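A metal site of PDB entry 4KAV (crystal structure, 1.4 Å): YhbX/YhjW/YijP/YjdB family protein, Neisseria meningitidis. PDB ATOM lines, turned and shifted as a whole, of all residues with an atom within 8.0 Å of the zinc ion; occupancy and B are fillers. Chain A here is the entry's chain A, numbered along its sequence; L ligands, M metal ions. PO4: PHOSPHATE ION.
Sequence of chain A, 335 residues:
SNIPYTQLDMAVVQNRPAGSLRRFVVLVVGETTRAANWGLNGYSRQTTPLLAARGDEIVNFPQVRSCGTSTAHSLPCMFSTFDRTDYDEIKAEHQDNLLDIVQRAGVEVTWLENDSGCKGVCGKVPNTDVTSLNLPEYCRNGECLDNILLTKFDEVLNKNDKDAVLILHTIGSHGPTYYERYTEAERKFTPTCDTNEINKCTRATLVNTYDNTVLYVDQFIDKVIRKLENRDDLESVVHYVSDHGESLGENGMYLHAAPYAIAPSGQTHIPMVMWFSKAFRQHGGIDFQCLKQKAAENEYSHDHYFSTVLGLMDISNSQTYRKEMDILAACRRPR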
ATOM      1  N   VAL A  29      21.375  26.981   6.848  1.00  0.00           N
ATOM      2  CA  VAL A  29      21.931  25.760   7.365  1.00  0.00           C
ATOM      3  C   VAL A  29      21.091  25.380   8.564  1.00  0.00           C
ATOM      4  O   VAL A  29      21.139  26.043   9.620  1.00  0.00           O
ATOM      5  CB  VAL A  29      23.397  25.921   7.736  1.00  0.00           C
ATOM      6  CG1 VAL A  29      23.914  24.604   8.331  1.00  0.00           C
ATOM      7  CG2 VAL A  29      24.205  26.311   6.500  1.00  0.00           C
ATOM      8  N   GLY A  30      20.294  24.331   8.369  1.00  0.00           N
ATOM      9  CA  GLY A  30      19.408  23.836   9.394  1.00  0.00           C
ATOM     10  C   GLY A  30      20.121  23.009  10.425  1.00  0.00           C
ATOM     11  O   GLY A  30      21.310  22.793  10.354  1.00  0.00           O
ATOM     12  N   GLU A  31      19.352  22.534  11.375  1.00  0.00           N
ATOM     13  CA  GLU A  31      19.889  21.859  12.527  1.00  0.00           C
ATOM     14  C   GLU A  31      18.849  20.825  12.967  1.00  0.00           C
ATOM     15  O   GLU A  31      17.710  21.176  13.293  1.00  0.00           O
ATOM     16  CB  GLU A  31      20.111  22.924  13.635  1.00  0.00           C
ATOM     17  CG  GLU A  31      20.531  22.350  14.982  1.00  0.00           C
ATOM     18  CD  GLU A  31      21.763  21.468  14.876  1.00  0.00           C
ATOM     19  OE1 GLU A  31      21.664  20.251  15.022  1.00  0.00           O
ATOM     20  OE2 GLU A  31      22.864  21.971  14.700  1.00  0.00           O
ATOM     21  N   THR A  32      19.258  19.561  13.007  1.00  0.00           N
ATOM     22  CA  THR A  32      18.471  18.463  13.611  1.00  0.00           C
ATOM     23  C   THR A  32      17.167  18.034  12.901  1.00  0.00           C
ATOM     24  O   THR A  32      16.690  16.920  13.124  1.00  0.00           O
ATOM     25  CB  THR A  32      18.252  18.758  15.130  1.00  0.00           C
ATOM     26  OG1 THR A  32      19.536  18.807  15.792  1.00  0.00           O
ATOM     27  CG2 THR A  32      17.403  17.698  15.787  1.00  0.00           C
ATOM     28  N   THR A  33      16.591  18.872  12.051  1.00  0.00           N
ATOM     29  CA  THR A  33      15.390  18.545  11.314  1.00  0.00           C
ATOM     30  C   THR A  33      15.603  17.381  10.354  1.00  0.00           C
ATOM     31  O   THR A  33      16.562  17.354   9.594  1.00  0.00           O
ATOM     32  CB  THR A  33      14.953  19.782  10.537  1.00  0.00           C
ATOM     33  OG1 THR A  33      14.946  20.884  11.451  1.00  0.00           O
ATOM     34  CG2 THR A  33      13.563  19.602   9.902  1.00  0.00           C
ATOM     35  N   GLY A  68      27.409  13.790   8.203  1.00  0.00           N
ATOM     36  CA  GLY A  68      27.677  13.429   9.575  1.00  0.00           C
ATOM     37  C   GLY A  68      26.400  13.441  10.390  1.00  0.00           C
ATOM     38  O   GLY A  68      25.329  13.726   9.852  1.00  0.00           O
ATOM     39  N   THR A  69      26.516  13.132  11.689  1.00  0.00           N
ATOM     40  CA  THR A  69      25.352  13.130  12.576  1.00  0.00           C
ATOM     41  C   THR A  69      25.530  14.160  13.680  1.00  0.00           C
ATOM     42  O   THR A  69      24.791  14.158  14.661  1.00  0.00           O
ATOM     43  CB  THR A  69      25.117  11.759  13.172  1.00  0.00           C
ATOM     44  OG1 THR A  69      26.293  11.377  13.889  1.00  0.00           O
ATOM     45  CG2 THR A  69      24.797  10.769  12.086  1.00  0.00           C
ATOM     46  N   SER A  70      26.463  15.093  13.499  1.00  0.00           N
ATOM     47  CA  SER A  70      26.630  16.177  14.444  1.00  0.00           C
ATOM     48  C   SER A  70      27.201  17.348  13.693  1.00  0.00           C
ATOM     49  O   SER A  70      27.759  17.167  12.623  1.00  0.00           O
ATOM     50  CB  SER A  70      27.595  15.797  15.579  1.00  0.00           C
ATOM     51  OG  SER A  70      28.896  15.524  15.074  1.00  0.00           O
ATOM     52  N   TPO A  71      27.027  18.587  14.163  1.00  0.00           N
ATOM     53  CA  TPO A  71      27.608  19.777  13.433  1.00  0.00           C
ATOM     54  CB  TPO A  71      27.468  21.207  14.058  1.00  0.00           C
ATOM     55  CG2 TPO A  71      26.023  21.608  14.144  1.00  0.00           C
ATOM     56  OG1 TPO A  71      28.100  21.323  15.337  1.00  0.00           O
ATOM     57  C   TPO A  71      29.108  19.655  13.312  1.00  0.00           C
ATOM     58  O   TPO A  71      29.694  20.061  12.284  1.00  0.00           O
ATOM     59  N   ALA A  72      29.752  19.165  14.359  1.00  0.00           N
ATOM     60  CA  ALA A  72      31.207  19.136  14.319  1.00  0.00           C
ATOM     61  C   ALA A  72      31.744  18.394  13.093  1.00  0.00           C
ATOM     62  O   ALA A  72      32.813  18.709  12.614  1.00  0.00           O
ATOM     63  CB  ALA A  72      31.740  18.485  15.594  1.00  0.00           C
ATOM     64  N   SER A  74      29.396  17.434  10.203  1.00  0.00           N
ATOM     65  CA  SER A  74      28.671  17.836   9.032  1.00  0.00           C
ATOM     66  C   SER A  74      29.076  19.184   8.460  1.00  0.00           C
ATOM     67  O   SER A  74      29.207  19.316   7.272  1.00  0.00           O
ATOM     68  CB  SER A  74      27.177  17.877   9.295  1.00  0.00           C
ATOM     69  OG  SER A  74      26.702  16.560   9.370  1.00  0.00           O
ATOM     70  N   LEU A  75      29.214  20.192   9.302  1.00  0.00           N
ATOM     71  CA  LEU A  75      29.526  21.514   8.785  1.00  0.00           C
ATOM     72  C   LEU A  75      30.883  21.573   8.067  1.00  0.00           C
ATOM     73  O   LEU A  75      30.941  22.043   6.925  1.00  0.00           O
ATOM     74  CB  LEU A  75      29.441  22.605   9.862  1.00  0.00           C
ATOM     75  CG  LEU A  75      28.130  23.393   9.776  1.00  0.00           C
ATOM     76  CD1 LEU A  75      26.921  22.459  10.007  1.00  0.00           C
ATOM     77  CD2 LEU A  75      28.114  24.566  10.758  1.00  0.00           C
ATOM     78  N   ASP A 115      23.339  29.136  16.319  1.00  0.00           N
ATOM     79  CA  ASP A 115      23.346  27.715  16.669  1.00  0.00           C
ATOM     80  C   ASP A 115      24.624  27.328  17.413  1.00  0.00           C
ATOM     81  O   ASP A 115      25.146  26.225  17.195  1.00  0.00           O
ATOM     82  CB  ASP A 115      23.230  26.879  15.387  1.00  0.00           C
ATOM     83  CG  ASP A 115      22.985  25.378  15.632  1.00  0.00           C
ATOM     84  OD1 ASP A 115      22.327  24.966  16.599  1.00  0.00           O
ATOM     85  OD2 ASP A 115      23.444  24.614  14.750  1.00  0.00           O
ATOM     86  N   LYS A 119      31.855  25.924  13.755  1.00  0.00           N
ATOM     87  CA  LYS A 119      32.826  24.817  13.693  1.00  0.00           C
ATOM     88  C   LYS A 119      34.003  25.127  12.780  1.00  0.00           C
ATOM     89  O   LYS A 119      34.494  24.272  12.036  1.00  0.00           O
ATOM     90  CB  LYS A 119      32.123  23.515  13.279  1.00  0.00           C
ATOM     91  CG  LYS A 119      31.089  23.034  14.306  1.00  0.00           C
ATOM     92  CD  LYS A 119      31.772  22.792  15.655  1.00  0.00           C
ATOM     93  CE  LYS A 119      30.872  22.094  16.698  1.00  0.00           C
ATOM     94  NZ  LYS A 119      29.863  23.010  17.338  1.00  0.00           N
ATOM     95  N   HIS A 169      22.724  30.362   9.985  1.00  0.00           N
ATOM     96  CA  HIS A 169      22.901  29.106  10.706  1.00  0.00           C
ATOM     97  C   HIS A 169      21.941  29.053  11.869  1.00  0.00           C
ATOM     98  O   HIS A 169      22.104  29.735  12.879  1.00  0.00           O
ATOM     99  CB  HIS A 169      24.319  28.970  11.197  1.00  0.00           C
ATOM    100  CG  HIS A 169      24.630  27.604  11.707  1.00  0.00           C
ATOM    101  ND1 HIS A 169      25.682  27.331  12.545  1.00  0.00           N
ATOM    102  CD2 HIS A 169      23.988  26.439  11.513  1.00  0.00           C
ATOM    103  CE1 HIS A 169      25.666  26.047  12.854  1.00  0.00           C
ATOM    104  NE2 HIS A 169      24.657  25.476  12.229  1.00  0.00           N
ATOM    105  N   THR A 170      20.924  28.207  11.726  1.00  0.00           N
ATOM    106  CA  THR A 170      19.777  28.173  12.605  1.00  0.00           C
ATOM    107  C   THR A 170      19.917  27.099  13.638  1.00  0.00           C
ATOM    108  O   THR A 170      20.620  26.133  13.423  1.00  0.00           O
ATOM    109  CB  THR A 170      18.464  27.856  11.812  1.00  0.00           C
ATOM    110  OG1 THR A 170      18.581  26.570  11.183  1.00  0.00           O
ATOM    111  CG2 THR A 170      18.167  28.909  10.804  1.00  0.00           C
ATOM    112  N   ILE A 171      19.221  27.277  14.764  1.00  0.00           N
ATOM    113  CA  ILE A 171      19.148  26.245  15.792  1.00  0.00           C
ATOM    114  C   ILE A 171      18.037  25.216  15.487  1.00  0.00           C
ATOM    115  O   ILE A 171      18.089  24.099  15.985  1.00  0.00           O
ATOM    116  CB  ILE A 171      19.013  26.869  17.201  1.00  0.00           C
ATOM    117  CG1 ILE A 171      19.154  25.798  18.287  1.00  0.00           C
ATOM    118  CG2 ILE A 171      17.725  27.597  17.373  1.00  0.00           C
ATOM    119  CD1 ILE A 171      19.402  26.353  19.673  1.00  0.00           C
ATOM    120  N   HIS A 174      16.840  21.643  17.270  1.00  0.00           N
ATOM    121  CA  HIS A 174      17.748  21.152  18.303  1.00  0.00           C
ATOM    122  C   HIS A 174      17.017  20.840  19.603  1.00  0.00           C
ATOM    123  O   HIS A 174      16.149  21.609  20.078  1.00  0.00           O
ATOM    124  CB  HIS A 174      18.853  22.182  18.566  1.00  0.00           C
ATOM    125  CG  HIS A 174      20.166  21.555  18.922  1.00  0.00           C
ATOM    126  ND1 HIS A 174      20.339  20.729  20.015  1.00  0.00           N
ATOM    127  CD2 HIS A 174      21.373  21.619  18.316  1.00  0.00           C
ATOM    128  CE1 HIS A 174      21.594  20.314  20.064  1.00  0.00           C
ATOM    129  NE2 HIS A 174      22.237  20.832  19.037  1.00  0.00           N
ATOM    130  N   SER A 242      19.390  20.645   6.266  1.00  0.00           N
ATOM    131  CA  SER A 242      19.748  20.397   7.649  1.00  0.00           C
ATOM    132  C   SER A 242      21.150  19.790   7.741  1.00  0.00           C
ATOM    133  O   SER A 242      21.635  19.209   6.783  1.00  0.00           O
ATOM    134  CB  SER A 242      18.753  19.405   8.230  1.00  0.00           C
ATOM    135  OG  SER A 242      18.886  19.383   9.634  1.00  0.00           O
ATOM    136  N   ASP A 243      21.783  19.873   8.907  1.00  0.00           N
ATOM    137  CA  ASP A 243      23.095  19.240   9.125  1.00  0.00           C
ATOM    138  C   ASP A 243      23.030  17.727   9.378  1.00  0.00           C
ATOM    139  O   ASP A 243      23.993  17.034   9.089  1.00  0.00           O
ATOM    140  CB  ASP A 243      23.913  19.915  10.252  1.00  0.00           C
ATOM    141  CG  ASP A 243      23.280  19.836  11.623  1.00  0.00           C
ATOM    142  OD1 ASP A 243      22.066  19.618  11.754  1.00  0.00           O
ATOM    143  OD2 ASP A 243      24.056  20.059  12.577  1.00  0.00           O
ATOM    144  N   HIS A 244      21.899  17.268   9.903  1.00  0.00           N
ATOM    145  CA  HIS A 244      21.628  15.863  10.187  1.00  0.00           C
ATOM    146  C   HIS A 244      20.221  15.833  10.802  1.00  0.00           C
ATOM    147  O   HIS A 244      19.618  16.886  11.063  1.00  0.00           O
ATOM    148  CB  HIS A 244      22.641  15.286  11.219  1.00  0.00           C
ATOM    149  CG  HIS A 244      22.693  16.103  12.477  1.00  0.00           C
ATOM    150  ND1 HIS A 244      21.673  16.084  13.409  1.00  0.00           N
ATOM    151  CD2 HIS A 244      23.566  17.066  12.886  1.00  0.00           C
ATOM    152  CE1 HIS A 244      21.920  16.978  14.345  1.00  0.00           C
ATOM    153  NE2 HIS A 244      23.058  17.584  14.057  1.00  0.00           N
ATOM    154  N   GLY A 245      19.724  14.627  11.061  1.00  0.00           N
ATOM    155  CA  GLY A 245      18.422  14.430  11.676  1.00  0.00           C
ATOM    156  C   GLY A 245      18.499  14.126  13.161  1.00  0.00           C
ATOM    157  O   GLY A 245      19.364  14.617  13.887  1.00  0.00           O
ATOM    158  N   GLU A 246      17.552  13.326  13.631  1.00  0.00           N
ATOM    159  CA  GLU A 246      17.347  13.146  15.057  1.00  0.00           C
ATOM    160  C   GLU A 246      16.694  11.787  15.272  1.00  0.00           C
ATOM    161  O   GLU A 246      15.955  11.324  14.402  1.00  0.00           O
ATOM    162  CB  GLU A 246      16.381  14.218  15.549  1.00  0.00           C
ATOM    163  CG  GLU A 246      16.246  14.399  17.044  1.00  0.00           C
ATOM    164  CD  GLU A 246      17.491  14.986  17.726  1.00  0.00           C
ATOM    165  OE1 GLU A 246      18.591  14.854  17.206  1.00  0.00           O
ATOM    166  OE2 GLU A 246      17.323  15.607  18.824  1.00  0.00           O
ATOM    167  N   HIS A 256      21.076  12.887  18.719  1.00  0.00           N
ATOM    168  CA  HIS A 256      21.779  12.530  17.478  1.00  0.00           C
ATOM    169  C   HIS A 256      23.207  12.128  17.789  1.00  0.00           C
ATOM    170  O   HIS A 256      23.430  11.498  18.824  1.00  0.00           O
ATOM    171  CB  HIS A 256      21.649  13.640  16.422  1.00  0.00           C
ATOM    172  CG  HIS A 256      21.992  15.013  16.906  1.00  0.00           C
ATOM    173  ND1 HIS A 256      21.056  15.860  17.444  1.00  0.00           N
ATOM    174  CD2 HIS A 256      23.173  15.687  16.937  1.00  0.00           C
ATOM    175  CE1 HIS A 256      21.633  16.999  17.780  1.00  0.00           C
ATOM    176  NE2 HIS A 256      22.917  16.916  17.499  1.00  0.00           N
ATOM    177  N   ALA A 257      24.137  12.407  16.881  1.00  0.00           N
ATOM    178  CA  ALA A 257      25.532  12.052  17.051  1.00  0.00           C
ATOM    179  C   ALA A 257      25.811  10.556  17.164  1.00  0.00           C
ATOM    180  O   ALA A 257      26.853  10.159  17.687  1.00  0.00           O
ATOM    181  CB  ALA A 257      26.135  12.820  18.242  1.00  0.00           C
HETATM  182  P   PO4 L   1      25.228  19.867  17.128  1.00  0.00           P
HETATM  183  O1  PO4 L   1      24.838  19.544  15.688  1.00  0.00           O
HETATM  184  O2  PO4 L   1      26.718  20.031  17.297  1.00  0.00           O
HETATM  185  O3  PO4 L   1      24.551  21.163  17.462  1.00  0.00           O
HETATM  186  O4  PO4 L   1      24.717  18.874  18.147  1.00  0.00           O
HETATM  187 ZN    ZN M   1      23.476  19.558  14.447  1.00  0.00          ZN
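The zinc ion is bound by O1 of the ligand (1.8 Å), OD2 of Asp 243 (2.0 Å), OE1 of Glu 31 (2.0 Å), NE2 of His 244 (2.1 Å) and OE2 of Glu 31 (2.5 Å).
The zinc ion has five donor atoms within binding distance.
TPO 71 touches the zinc ion.
Four residues have an atom within 4 Å of the zinc ion: Glu 31, TPO 71, Asp 243 and His 244.
Along chain A the residues within 4 Å of the zinc ion span positions 31 to 244.
The backbone carbonyl oxygen (O) of Glu 31 lies within hydrogen-bond range of the side-chain hydroxyl (OG1) of Thr 33 (3.3 Å).
The side-chain hydroxyl (OG) of Ser 242 is in hydrogen-bond range of the backbone carbonyl oxygen (O) of His 244 (3.0 Å).
The side-chain amino group (NZ) of Lys 119 lies within hydrogen-bond range of OG1 of TPO 71 (3.2 Å).
O of Asp 243 sits at hydrogen-bond distance from OG of Ser 74 (2.8 Å).
OD1 of Asp 243 is in hydrogen-bond range of N of Thr 32.
The backbone carbonyl oxygen (O) of His 244 lies close to the backbone NH (N) of Thr 32 (3.3 Å).
The side-chain carboxylate (OE2) of Glu 31 sits close to the side-chain carboxylate (OD2) of Asp 115 (2.7 Å).
O of Gly 30 is in hydrogen-bond range of N of Asp 243 (3.3 Å).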
